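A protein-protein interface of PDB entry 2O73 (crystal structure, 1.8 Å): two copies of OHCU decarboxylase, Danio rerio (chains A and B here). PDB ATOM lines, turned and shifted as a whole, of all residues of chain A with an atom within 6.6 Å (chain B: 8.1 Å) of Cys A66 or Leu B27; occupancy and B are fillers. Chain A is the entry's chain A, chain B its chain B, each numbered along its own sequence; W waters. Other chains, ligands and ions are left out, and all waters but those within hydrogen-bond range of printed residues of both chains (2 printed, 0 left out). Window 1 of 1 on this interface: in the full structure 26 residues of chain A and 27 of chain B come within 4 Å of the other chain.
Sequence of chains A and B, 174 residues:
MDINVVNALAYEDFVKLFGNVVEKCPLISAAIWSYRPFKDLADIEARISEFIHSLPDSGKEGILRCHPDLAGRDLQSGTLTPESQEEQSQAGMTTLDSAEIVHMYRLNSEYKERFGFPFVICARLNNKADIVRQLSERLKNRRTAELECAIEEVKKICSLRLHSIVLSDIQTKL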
ATOM      1  N   GLU A  23      -6.433   5.784  18.884  1.00  0.00           N
ATOM      2  CA  GLU A  23      -7.553   6.613  19.359  1.00  0.00           C
ATOM      3  C   GLU A  23      -8.325   6.061  20.565  1.00  0.00           C
ATOM      4  O   GLU A  23      -8.906   4.974  20.487  1.00  0.00           O
ATOM      5  CB  GLU A  23      -8.538   6.881  18.207  1.00  0.00           C
ATOM      6  CG  GLU A  23      -9.722   7.780  18.599  1.00  0.00           C
ATOM      7  CD  GLU A  23      -9.388   9.270  18.649  1.00  0.00           C
ATOM      8  OE1 GLU A  23      -8.188   9.647  18.700  1.00  0.00           O
ATOM      9  OE2 GLU A  23     -10.342  10.090  18.641  1.00  0.00           O
ATOM     10  N   LYS A  24      -8.350   6.850  21.644  1.00  0.00           N
ATOM     11  CA  LYS A  24      -9.048   6.536  22.898  1.00  0.00           C
ATOM     12  C   LYS A  24      -8.652   5.172  23.484  1.00  0.00           C
ATOM     13  O   LYS A  24      -9.443   4.514  24.158  1.00  0.00           O
ATOM     14  CB  LYS A  24     -10.574   6.682  22.730  1.00  0.00           C
ATOM     15  CG  LYS A  24     -10.979   8.118  22.374  1.00  0.00           C
ATOM     16  CD  LYS A  24     -12.485   8.297  22.279  1.00  0.00           C
ATOM     17  CE  LYS A  24     -12.841   9.695  21.799  1.00  0.00           C
ATOM     18  NZ  LYS A  24     -14.316   9.855  21.692  1.00  0.00           N
ATOM     19  N   CYS A  25      -7.413   4.760  23.220  1.00  0.00           N
ATOM     20  CA  CYS A  25      -6.906   3.489  23.714  1.00  0.00           C
ATOM     21  C   CYS A  25      -5.549   3.676  24.419  1.00  0.00           C
ATOM     22  O   CYS A  25      -4.532   3.103  24.005  1.00  0.00           O
ATOM     23  CB  CYS A  25      -6.793   2.469  22.573  1.00  0.00           C
ATOM     24  SG  CYS A  25      -8.370   1.984  21.798  1.00  0.00           S
ATOM     25  N   LEU A  27      -4.658   2.384  26.982  1.00  0.00           N
ATOM     26  CA  LEU A  27      -4.240   1.096  27.486  1.00  0.00           C
ATOM     27  C   LEU A  27      -3.093   0.498  26.673  1.00  0.00           C
ATOM     28  O   LEU A  27      -2.178  -0.115  27.222  1.00  0.00           O
ATOM     29  CB  LEU A  27      -5.428   0.134  27.488  1.00  0.00           C
ATOM     30  CG  LEU A  27      -4.949  -1.303  27.564  1.00  0.00           C
ATOM     31  CD1 LEU A  27      -4.450  -1.532  28.977  1.00  0.00           C
ATOM     32  CD2 LEU A  27      -6.041  -2.281  27.199  1.00  0.00           C
ATOM     33  N   ILE A  28      -3.140   0.662  25.356  1.00  0.00           N
ATOM     34  CA  ILE A  28      -2.104   0.103  24.507  1.00  0.00           C
ATOM     35  C   ILE A  28      -0.757   0.798  24.731  1.00  0.00           C
ATOM     36  O   ILE A  28       0.257   0.138  24.878  1.00  0.00           O
ATOM     37  CB  ILE A  28      -2.496   0.181  23.028  1.00  0.00           C
ATOM     38  CG1 ILE A  28      -3.902  -0.416  22.831  1.00  0.00           C
ATOM     39  CG2 ILE A  28      -1.444  -0.522  22.164  1.00  0.00           C
ATOM     40  CD1 ILE A  28      -4.408  -0.278  21.432  1.00  0.00           C
ATOM     41  N   PHE A  51       0.954  -6.135  20.274  1.00  0.00           N
ATOM     42  CA  PHE A  51      -0.077  -6.077  21.292  1.00  0.00           C
ATOM     43  C   PHE A  51      -1.444  -6.215  20.640  1.00  0.00           C
ATOM     44  O   PHE A  51      -2.274  -7.008  21.082  1.00  0.00           O
ATOM     45  CB  PHE A  51      -0.013  -4.776  22.089  1.00  0.00           C
ATOM     46  CG  PHE A  51      -0.981  -4.745  23.246  1.00  0.00           C
ATOM     47  CD1 PHE A  51      -0.642  -5.316  24.465  1.00  0.00           C
ATOM     48  CD2 PHE A  51      -2.233  -4.164  23.105  1.00  0.00           C
ATOM     49  CE1 PHE A  51      -1.550  -5.309  25.519  1.00  0.00           C
ATOM     50  CE2 PHE A  51      -3.149  -4.156  24.156  1.00  0.00           C
ATOM     51  CZ  PHE A  51      -2.800  -4.730  25.360  1.00  0.00           C
ATOM     52  N   LEU A  55      -4.611  -9.568  20.663  1.00  0.00           N
ATOM     53  CA  LEU A  55      -5.969  -9.462  21.185  1.00  0.00           C
ATOM     54  C   LEU A  55      -6.878 -10.440  20.460  1.00  0.00           C
ATOM     55  O   LEU A  55      -6.579 -10.840  19.340  1.00  0.00           O
ATOM     56  CB  LEU A  55      -6.512  -8.044  21.009  1.00  0.00           C
ATOM     57  CG  LEU A  55      -5.763  -6.915  21.706  1.00  0.00           C
ATOM     58  CD1 LEU A  55      -6.278  -5.570  21.185  1.00  0.00           C
ATOM     59  CD2 LEU A  55      -5.930  -7.026  23.221  1.00  0.00           C
ATOM     60  N   SER A  58     -12.501  -9.709  18.992  1.00  0.00           N
ATOM     61  CA  SER A  58     -13.364  -8.735  19.683  1.00  0.00           C
ATOM     62  C   SER A  58     -12.594  -7.493  20.148  1.00  0.00           C
ATOM     63  O   SER A  58     -13.142  -6.404  20.135  1.00  0.00           O
ATOM     64  CB  SER A  58     -14.115  -9.370  20.860  1.00  0.00           C
ATOM     65  OG  SER A  58     -13.223  -9.821  21.866  1.00  0.00           O
ATOM     66  N   GLY A  59     -11.345  -7.671  20.576  1.00  0.00           N
ATOM     67  CA  GLY A  59     -10.477  -6.543  20.955  1.00  0.00           C
ATOM     68  C   GLY A  59     -10.159  -5.625  19.786  1.00  0.00           C
ATOM     69  O   GLY A  59     -10.185  -4.405  19.919  1.00  0.00           O
ATOM     70  N   LYS A  60      -9.841  -6.221  18.640  1.00  0.00           N
ATOM     71  CA  LYS A  60      -9.585  -5.461  17.420  1.00  0.00           C
ATOM     72  C   LYS A  60     -10.831  -4.672  16.999  1.00  0.00           C
ATOM     73  O   LYS A  60     -10.745  -3.484  16.752  1.00  0.00           O
ATOM     74  CB  LYS A  60      -9.099  -6.386  16.310  1.00  0.00           C
ATOM     75  CG  LYS A  60      -7.672  -6.886  16.554  1.00  0.00           C
ATOM     76  CD  LYS A  60      -7.314  -8.051  15.661  1.00  0.00           C
ATOM     77  CE  LYS A  60      -6.086  -8.758  16.231  1.00  0.00           C
ATOM     78  NZ  LYS A  60      -5.593  -9.856  15.364  1.00  0.00           N
ATOM     79  N   GLU A  61     -11.987  -5.317  16.995  1.00  0.00           N
ATOM     80  CA  GLU A  61     -13.264  -4.598  16.767  1.00  0.00           C
ATOM     81  C   GLU A  61     -13.460  -3.483  17.789  1.00  0.00           C
ATOM     82  O   GLU A  61     -13.880  -2.368  17.451  1.00  0.00           O
ATOM     83  CB  GLU A  61     -14.459  -5.555  16.836  1.00  0.00           C
ATOM     84  CG  GLU A  61     -14.395  -6.691  15.845  1.00  0.00           C
ATOM     85  CD  GLU A  61     -15.519  -7.694  16.044  1.00  0.00           C
ATOM     86  OE1 GLU A  61     -15.665  -8.259  17.160  1.00  0.00           O
ATOM     87  OE2 GLU A  61     -16.258  -7.921  15.074  1.00  0.00           O
ATOM     88  N   GLY A  62     -13.172  -3.800  19.048  1.00  0.00           N
ATOM     89  CA  GLY A  62     -13.313  -2.848  20.120  1.00  0.00           C
ATOM     90  C   GLY A  62     -12.485  -1.604  19.840  1.00  0.00           C
ATOM     91  O   GLY A  62     -12.945  -0.493  20.090  1.00  0.00           O
ATOM     92  N   ILE A  63     -11.261  -1.788  19.322  1.00  0.00           N
ATOM     93  CA  ILE A  63     -10.377  -0.649  19.026  1.00  0.00           C
ATOM     94  C   ILE A  63     -11.032   0.272  17.993  1.00  0.00           C
ATOM     95  O   ILE A  63     -11.118   1.507  18.164  1.00  0.00           O
ATOM     96  CB  ILE A  63      -8.969  -1.127  18.549  1.00  0.00           C
ATOM     97  CG1 ILE A  63      -8.180  -1.728  19.729  1.00  0.00           C
ATOM     98  CG2 ILE A  63      -8.160   0.034  17.932  1.00  0.00           C
ATOM     99  CD1 ILE A  63      -6.874  -2.342  19.320  1.00  0.00           C
ATOM    100  N   LEU A  64     -11.509  -0.347  16.925  1.00  0.00           N
ATOM    101  CA  LEU A  64     -12.205   0.355  15.853  1.00  0.00           C
ATOM    102  C   LEU A  64     -13.413   1.150  16.393  1.00  0.00           C
ATOM    103  O   LEU A  64     -13.661   2.306  16.006  1.00  0.00           O
ATOM    104  CB  LEU A  64     -12.636  -0.662  14.797  1.00  0.00           C
ATOM    105  CG  LEU A  64     -11.505  -1.418  14.079  1.00  0.00           C
ATOM    106  CD1 LEU A  64     -12.043  -2.491  13.147  1.00  0.00           C
ATOM    107  CD2 LEU A  64     -10.576  -0.455  13.330  1.00  0.00           C
ATOM    108  N   ARG A  65     -14.136   0.537  17.324  1.00  0.00           N
ATOM    109  CA  ARG A  65     -15.316   1.162  17.924  1.00  0.00           C
ATOM    110  C   ARG A  65     -14.965   2.353  18.812  1.00  0.00           C
ATOM    111  O   ARG A  65     -15.839   3.128  19.179  1.00  0.00           O
ATOM    112  CB  ARG A  65     -16.144   0.128  18.696  1.00  0.00           C
ATOM    113  CG  ARG A  65     -16.861  -0.883  17.809  1.00  0.00           C
ATOM    114  CD  ARG A  65     -17.432  -2.031  18.620  1.00  0.00           C
ATOM    115  NE  ARG A  65     -17.778  -3.113  17.732  1.00  0.00           N
ATOM    116  CZ  ARG A  65     -17.696  -4.407  18.002  1.00  0.00           C
ATOM    117  NH1 ARG A  65     -17.287  -4.848  19.179  1.00  0.00           N
ATOM    118  NH2 ARG A  65     -18.049  -5.271  17.066  1.00  0.00           N
ATOM    119  N   CYS A  66     -13.683   2.512  19.143  1.00  0.00           N
ATOM    120  CA  CYS A  66     -13.249   3.670  19.902  1.00  0.00           C
ATOM    121  C   CYS A  66     -12.958   4.868  18.987  1.00  0.00           C
ATOM    122  O   CYS A  66     -12.664   5.950  19.478  1.00  0.00           O
ATOM    123  CB  CYS A  66     -12.014   3.340  20.760  1.00  0.00           C
ATOM    124  SG  CYS A  66     -12.401   2.276  22.168  1.00  0.00           S
ATOM    125  N   HIS A  67     -13.022   4.669  17.673  1.00  0.00           N
ATOM    126  CA  HIS A  67     -12.747   5.746  16.720  1.00  0.00           C
ATOM    127  C   HIS A  67     -14.027   6.519  16.374  1.00  0.00           C
ATOM    128  O   HIS A  67     -15.100   5.931  16.258  1.00  0.00           O
ATOM    129  CB  HIS A  67     -12.122   5.201  15.437  1.00  0.00           C
ATOM    130  CG  HIS A  67     -10.692   4.775  15.581  1.00  0.00           C
ATOM    131  ND1 HIS A  67     -10.319   3.595  16.197  1.00  0.00           N
ATOM    132  CD2 HIS A  67      -9.542   5.367  15.173  1.00  0.00           C
ATOM    133  CE1 HIS A  67      -9.002   3.483  16.161  1.00  0.00           C
ATOM    134  NE2 HIS A  67      -8.509   4.540  15.540  1.00  0.00           N
ATOM    135  N   PRO A  68     -13.915   7.842  16.221  1.00  0.00           N
ATOM    136  CA  PRO A  68     -15.101   8.579  15.811  1.00  0.00           C
ATOM    137  C   PRO A  68     -15.345   8.452  14.319  1.00  0.00           C
ATOM    138  O   PRO A  68     -14.431   8.130  13.571  1.00  0.00           O
ATOM    139  CB  PRO A  68     -14.759  10.024  16.172  1.00  0.00           C
ATOM    140  CG  PRO A  68     -13.258  10.097  16.073  1.00  0.00           C
ATOM    141  CD  PRO A  68     -12.745   8.723  16.438  1.00  0.00           C
ATOM    142  N   PRO A 118     -17.009   1.203  13.191  1.00  0.00           N
ATOM    143  CA  PRO A 118     -16.914   2.351  12.287  1.00  0.00           C
ATOM    144  C   PRO A 118     -16.003   2.090  11.113  1.00  0.00           C
ATOM    145  O   PRO A 118     -15.111   1.228  11.172  1.00  0.00           O
ATOM    146  CB  PRO A 118     -16.325   3.459  13.162  1.00  0.00           C
ATOM    147  CG  PRO A 118     -16.487   2.962  14.611  1.00  0.00           C
ATOM    148  CD  PRO A 118     -16.397   1.471  14.503  1.00  0.00           C
ATOM    149  N   TYR B  11     -23.676   0.126  18.905  1.00  0.00           N
ATOM    150  CA  TYR B  11     -22.397   0.038  19.606  1.00  0.00           C
ATOM    151  C   TYR B  11     -21.980   1.424  20.105  1.00  0.00           C
ATOM    152  O   TYR B  11     -21.412   1.543  21.180  1.00  0.00           O
ATOM    153  CB  TYR B  11     -21.300  -0.645  18.771  1.00  0.00           C
ATOM    154  CG  TYR B  11     -20.843   0.130  17.547  1.00  0.00           C
ATOM    155  CD1 TYR B  11     -21.168  -0.314  16.262  1.00  0.00           C
ATOM    156  CD2 TYR B  11     -20.079   1.300  17.678  1.00  0.00           C
ATOM    157  CE1 TYR B  11     -20.735   0.381  15.135  1.00  0.00           C
ATOM    158  CE2 TYR B  11     -19.656   2.019  16.548  1.00  0.00           C
ATOM    159  CZ  TYR B  11     -19.987   1.540  15.285  1.00  0.00           C
ATOM    160  OH  TYR B  11     -19.613   2.223  14.150  1.00  0.00           O
ATOM    161  N   VAL B  15     -21.065   1.857  23.995  1.00  0.00           N
ATOM    162  CA  VAL B  15     -19.755   2.367  24.415  1.00  0.00           C
ATOM    163  C   VAL B  15     -19.916   3.641  25.257  1.00  0.00           C
ATOM    164  O   VAL B  15     -19.205   3.824  26.242  1.00  0.00           O
ATOM    165  CB  VAL B  15     -18.796   2.586  23.210  1.00  0.00           C
ATOM    166  CG1 VAL B  15     -17.452   3.175  23.667  1.00  0.00           C
ATOM    167  CG2 VAL B  15     -18.552   1.265  22.461  1.00  0.00           C
ATOM    168  N   PHE B  18     -21.314   2.273  28.703  1.00  0.00           N
ATOM    169  CA  PHE B  18     -20.451   1.319  29.420  1.00  0.00           C
ATOM    170  C   PHE B  18     -18.949   1.590  29.264  1.00  0.00           C
ATOM    171  O   PHE B  18     -18.133   0.825  29.760  1.00  0.00           O
ATOM    172  CB  PHE B  18     -20.722  -0.108  28.936  1.00  0.00           C
ATOM    173  CG  PHE B  18     -22.086  -0.650  29.310  1.00  0.00           C
ATOM    174  CD1 PHE B  18     -22.290  -1.273  30.536  1.00  0.00           C
ATOM    175  CD2 PHE B  18     -23.153  -0.554  28.433  1.00  0.00           C
ATOM    176  CE1 PHE B  18     -23.541  -1.785  30.887  1.00  0.00           C
ATOM    177  CE2 PHE B  18     -24.403  -1.067  28.780  1.00  0.00           C
ATOM    178  CZ  PHE B  18     -24.592  -1.673  30.011  1.00  0.00           C
ATOM    179  N   GLY B  19     -18.594   2.650  28.556  1.00  0.00           N
ATOM    180  CA  GLY B  19     -17.198   2.913  28.208  1.00  0.00           C
ATOM    181  C   GLY B  19     -16.235   3.207  29.351  1.00  0.00           C
ATOM    182  O   GLY B  19     -15.030   3.170  29.151  1.00  0.00           O
ATOM    183  N   ASN B  20     -16.747   3.515  30.542  1.00  0.00           N
ATOM    184  CA  ASN B  20     -15.872   3.749  31.678  1.00  0.00           C
ATOM    185  C   ASN B  20     -16.030   2.754  32.841  1.00  0.00           C
ATOM    186  O   ASN B  20     -15.560   3.016  33.945  1.00  0.00           O
ATOM    187  CB  ASN B  20     -15.997   5.188  32.189  1.00  0.00           C
ATOM    188  CG  ASN B  20     -14.747   5.651  32.916  1.00  0.00           C
ATOM    189  OD1 ASN B  20     -14.809   6.162  34.040  1.00  0.00           O
ATOM    190  ND2 ASN B  20     -13.603   5.477  32.276  1.00  0.00           N
ATOM    191  N   VAL B  22     -14.429   0.098  33.088  1.00  0.00           N
ATOM    192  CA  VAL B  22     -13.012  -0.090  33.401  1.00  0.00           C
ATOM    193  C   VAL B  22     -12.345   1.250  33.118  1.00  0.00           C
ATOM    194  O   VAL B  22     -12.389   1.754  32.002  1.00  0.00           O
ATOM    195  CB  VAL B  22     -12.350  -1.248  32.618  1.00  0.00           C
ATOM    196  CG1 VAL B  22     -10.843  -1.344  32.953  1.00  0.00           C
ATOM    197  CG2 VAL B  22     -13.053  -2.568  32.932  1.00  0.00           C
ATOM    198  N   LYS B  24     -10.950   4.446  32.049  1.00  0.00           N
ATOM    199  CA  LYS B  24     -10.311   4.943  30.831  1.00  0.00           C
ATOM    200  C   LYS B  24      -9.998   3.861  29.808  1.00  0.00           C
ATOM    201  O   LYS B  24      -9.132   4.040  28.943  1.00  0.00           O
ATOM    202  CB  LYS B  24      -9.071   5.778  31.174  1.00  0.00           C
ATOM    203  CG  LYS B  24      -9.406   6.977  32.074  1.00  0.00           C
ATOM    204  CD  LYS B  24      -8.265   7.963  32.196  1.00  0.00           C
ATOM    205  CE  LYS B  24      -8.702   9.209  32.967  1.00  0.00           C
ATOM    206  NZ  LYS B  24      -7.700  10.334  32.853  1.00  0.00           N
ATOM    207  N   CYS B  25     -10.710   2.740  29.901  1.00  0.00           N
ATOM    208  CA  CYS B  25     -10.517   1.640  28.964  1.00  0.00           C
ATOM    209  C   CYS B  25     -11.807   1.296  28.213  1.00  0.00           C
ATOM    210  O   CYS B  25     -12.343   0.194  28.368  1.00  0.00           O
ATOM    211  CB  CYS B  25      -9.978   0.386  29.685  1.00  0.00           C
ATOM    212  SG  CYS B  25      -8.310   0.538  30.439  1.00  0.00           S
ATOM    213  N   PRO B  26     -12.307   2.232  27.391  1.00  0.00           N
ATOM    214  CA  PRO B  26     -13.545   1.950  26.648  1.00  0.00           C
ATOM    215  C   PRO B  26     -13.398   0.777  25.688  1.00  0.00           C
ATOM    216  O   PRO B  26     -14.396   0.129  25.330  1.00  0.00           O
ATOM    217  CB  PRO B  26     -13.814   3.252  25.883  1.00  0.00           C
ATOM    218  CG  PRO B  26     -12.447   3.940  25.795  1.00  0.00           C
ATOM    219  CD  PRO B  26     -11.770   3.572  27.105  1.00  0.00           C
ATOM    220  N   LEU B  27     -12.169   0.503  25.260  1.00  0.00           N
ATOM    221  CA  LEU B  27     -11.922  -0.614  24.363  1.00  0.00           C
ATOM    222  C   LEU B  27     -12.508  -1.911  24.910  1.00  0.00           C
ATOM    223  O   LEU B  27     -13.017  -2.749  24.157  1.00  0.00           O
ATOM    224  CB  LEU B  27     -10.415  -0.807  24.154  1.00  0.00           C
ATOM    225  CG  LEU B  27     -10.149  -2.259  23.787  1.00  0.00           C
ATOM    226  CD1 LEU B  27     -10.469  -2.419  22.287  1.00  0.00           C
ATOM    227  CD2 LEU B  27      -8.747  -2.709  24.128  1.00  0.00           C
ATOM    228  N   ILE B  28     -12.434  -2.076  26.225  1.00  0.00           N
ATOM    229  CA  ILE B  28     -12.887  -3.316  26.851  1.00  0.00           C
ATOM    230  C   ILE B  28     -14.401  -3.513  26.675  1.00  0.00           C
ATOM    231  O   ILE B  28     -14.844  -4.542  26.168  1.00  0.00           O
ATOM    232  CB  ILE B  28     -12.436  -3.381  28.335  1.00  0.00           C
ATOM    233  CG1 ILE B  28     -10.903  -3.580  28.412  1.00  0.00           C
ATOM    234  CG2 ILE B  28     -13.192  -4.476  29.068  1.00  0.00           C
ATOM    235  CD1 ILE B  28     -10.342  -3.627  29.840  1.00  0.00           C
ATOM    236  N   SER B  29     -15.179  -2.513  27.051  1.00  0.00           N
ATOM    237  CA  SER B  29     -16.625  -2.550  26.841  1.00  0.00           C
ATOM    238  C   SER B  29     -16.977  -2.613  25.352  1.00  0.00           C
ATOM    239  O   SER B  29     -17.902  -3.324  24.952  1.00  0.00           O
ATOM    240  CB  SER B  29     -17.260  -1.307  27.438  1.00  0.00           C
ATOM    241  OG  SER B  29     -17.269  -0.260  26.474  1.00  0.00           O
ATOM    242  N   ALA B  30     -16.252  -1.846  24.538  1.00  0.00           N
ATOM    243  CA  ALA B  30     -16.487  -1.839  23.094  1.00  0.00           C
ATOM    244  C   ALA B  30     -16.299  -3.250  22.532  1.00  0.00           C
ATOM    245  O   ALA B  30     -17.035  -3.677  21.653  1.00  0.00           O
ATOM    246  CB  ALA B  30     -15.552  -0.853  22.405  1.00  0.00           C
ATOM    247  N   ALA B  31     -15.301  -3.966  23.050  1.00  0.00           N
ATOM    248  CA  ALA B  31     -15.001  -5.329  22.620  1.00  0.00           C
ATOM    249  C   ALA B  31     -16.153  -6.283  22.916  1.00  0.00           C
ATOM    250  O   ALA B  31     -16.641  -6.998  22.029  1.00  0.00           O
ATOM    251  CB  ALA B  31     -13.738  -5.823  23.299  1.00  0.00           C
ATOM    252  N   ILE B  32     -16.603  -6.287  24.167  1.00  0.00           N
ATOM    253  CA  ILE B  32     -17.580  -7.290  24.585  1.00  0.00           C
ATOM    254  C   ILE B  32     -18.959  -7.106  23.925  1.00  0.00           C
ATOM    255  O   ILE B  32     -19.803  -7.995  24.001  1.00  0.00           O
ATOM    256  CB  ILE B  32     -17.686  -7.423  26.144  1.00  0.00           C
ATOM    257  CG1 ILE B  32     -18.128  -6.115  26.772  1.00  0.00           C
ATOM    258  CG2 ILE B  32     -16.378  -7.897  26.759  1.00  0.00           C
ATOM    259  CD1 ILE B  32     -19.606  -5.967  26.799  1.00  0.00           C
ATOM    260  N   TRP B  33     -19.185  -5.966  23.274  1.00  0.00           N
ATOM    261  CA  TRP B  33     -20.427  -5.749  22.504  1.00  0.00           C
ATOM    262  C   TRP B  33     -20.549  -6.748  21.350  1.00  0.00           C
ATOM    263  O   TRP B  33     -21.658  -7.058  20.885  1.00  0.00           O
ATOM    264  CB  TRP B  33     -20.492  -4.314  21.962  1.00  0.00           C
ATOM    265  CG  TRP B  33     -21.774  -3.926  21.230  1.00  0.00           C
ATOM    266  CD1 TRP B  33     -22.934  -3.466  21.795  1.00  0.00           C
ATOM    267  CD2 TRP B  33     -21.989  -3.899  19.804  1.00  0.00           C
ATOM    268  NE1 TRP B  33     -23.854  -3.170  20.819  1.00  0.00           N
ATOM    269  CE2 TRP B  33     -23.306  -3.438  19.591  1.00  0.00           C
ATOM    270  CE3 TRP B  33     -21.204  -4.243  18.691  1.00  0.00           C
ATOM    271  CZ2 TRP B  33     -23.855  -3.309  18.312  1.00  0.00           C
ATOM    272  CZ3 TRP B  33     -21.758  -4.115  17.412  1.00  0.00           C
ATOM    273  CH2 TRP B  33     -23.061  -3.640  17.238  1.00  0.00           C
ATOM    274  N   PHE B  51     -12.293 -11.226  28.892  1.00  0.00           N
ATOM    275  CA  PHE B  51     -11.469 -10.373  28.048  1.00  0.00           C
ATOM    276  C   PHE B  51     -10.201  -9.937  28.797  1.00  0.00           C
ATOM    277  O   PHE B  51      -9.078 -10.127  28.312  1.00  0.00           O
ATOM    278  CB  PHE B  51     -12.263  -9.148  27.556  1.00  0.00           C
ATOM    279  CG  PHE B  51     -11.497  -8.290  26.587  1.00  0.00           C
ATOM    280  CD1 PHE B  51     -11.576  -8.523  25.212  1.00  0.00           C
ATOM    281  CD2 PHE B  51     -10.687  -7.253  27.038  1.00  0.00           C
ATOM    282  CE1 PHE B  51     -10.856  -7.740  24.311  1.00  0.00           C
ATOM    283  CE2 PHE B  51      -9.954  -6.463  26.142  1.00  0.00           C
ATOM    284  CZ  PHE B  51     -10.053  -6.694  24.776  1.00  0.00           C
ATOM    285  N   LEU B  55      -5.745 -10.978  28.139  1.00  0.00           N
ATOM    286  CA  LEU B  55      -4.634 -10.048  27.857  1.00  0.00           C
ATOM    287  C   LEU B  55      -3.280 -10.545  28.342  1.00  0.00           C
ATOM    288  O   LEU B  55      -3.205 -11.201  29.379  1.00  0.00           O
ATOM    289  CB  LEU B  55      -4.898  -8.691  28.517  1.00  0.00           C
ATOM    290  CG  LEU B  55      -6.174  -7.948  28.144  1.00  0.00           C
ATOM    291  CD1 LEU B  55      -6.268  -6.635  28.938  1.00  0.00           C
ATOM    292  CD2 LEU B  55      -6.232  -7.687  26.622  1.00  0.00           C
ATOM    293  N   ILE B  63      -3.871  -1.624  31.872  1.00  0.00           N
ATOM    294  CA  ILE B  63      -5.140  -1.269  32.509  1.00  0.00           C
ATOM    295  C   ILE B  63      -4.903  -0.568  33.844  1.00  0.00           C
ATOM    296  O   ILE B  63      -5.497   0.467  34.109  1.00  0.00           O
ATOM    297  CB  ILE B  63      -6.029  -2.503  32.746  1.00  0.00           C
ATOM    298  CG1 ILE B  63      -6.533  -3.052  31.406  1.00  0.00           C
ATOM    299  CG2 ILE B  63      -7.196  -2.166  33.703  1.00  0.00           C
ATOM    300  CD1 ILE B  63      -7.231  -4.409  31.507  1.00  0.00           C
HETATM  301  O   HOH W   1      -9.673   2.047  25.251  1.00  0.00           O
HETATM  302  O   HOH W   2      -7.652   2.353  27.159  1.00  0.00           O
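The backbone carbonyl oxygen (O) of Ala B30 is in hydrogen-bond range of the guanidinium group (NH1) of Arg A65 (2.7 Å). The side-chain sulfur of Cys A66 sits at hydrogen-bond distance from the backbone NH of Leu B27, at 3.6 Å. The backbone nitrogen of Pro A118 sits close to the side-chain hydroxyl of Tyr B11 (3.0 Å).
The side-chain carboxylate (OE2) of Glu A61 lies within salt-bridge range of the guanidinium group (NH2) of Arg A65. O of Gly A62 lies within hydrogen-bond range of SG of Cys A66 (3.5 Å). The backbone carbonyl oxygen (O) of Ile A63 lies within hydrogen-bond range of a ring nitrogen (ND1) of His A67 (3.0 Å). O of Pro B26 sits at hydrogen-bond distance from OG of Ser B29, 3.1 Å away.
Ile B63 touches Leu A27. CB of Ala B31 touches O of Ser A58, at 3.3 Å. Leu B27 touches Gly A59 (CD1 to O, 3.1 Å). Gly A59 touches Phe B51 (CA to CE1, 3.6 Å). Ala B30 touches Gly A62. Gly A62 touches Ala B31. Ile A63 touches Leu B27 (N to CD1, 3.1 Å). Arg A65 touches Tyr B11 (CG to CD2, 3.9 Å). NH1 of Arg A65 touches O of Ala B31, at 3.6 Å. Cys A66 touches Pro B26.
Of the printed residues of chain B, Gly A59 touches Leu B27 and Phe B51. Printed residues of chain B within 4 Å of Ile A63: Leu B27. Of chain B, only Pro B26 and Leu B27 come within 4 Å of Cys A66. Leu B27 touches just these residues of chain A: Gly A59, Gly A62, Ile A63 and Cys A66. Printed residues of chain A within 4 Å of Phe B51: Ser A58 and Gly A59.
Hydrophobic or aromatic side chains of chain A within 4 Å of the printed part of chain B: Leu A27, Leu A55, Ile A63 and Pro A118. Along chain A the printed residues that touch a printed residue of chain B span positions 24 to 118. Printed residues of chain B that touch a printed residue of chain A: Tyr B11, Pro B26, Leu B27, Ala B30, Ala B31, Trp B33, Phe B51, Leu B55 and Ile B63. Hydrophobic or aromatic side chains of chain B that line the printed part of chain A: Tyr B11, Pro B26, Leu B27, Ala B30, Ala B31, Trp B33, Phe B51, Leu B55 and Ile B63.
Leu A27 touches Ile B63, and with the chains exchanged Ile A63 touches Leu B27. Leu B55 touches its own counterpart, Leu A55. Of the 18 pairs that touch across the chains among the printed residues, 3 have their exchanged pair printed and touching as well.
Water W1 lies within hydrogen-bond range of O of Lys A24 (2.7 Å), N of Leu B27 (2.9 Å) and SG of Cys A25 (3.7 Å). Water W2 bridges the backbone carbonyl oxygen (O) of Lys B24 and the backbone NH (N) of Leu A27.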
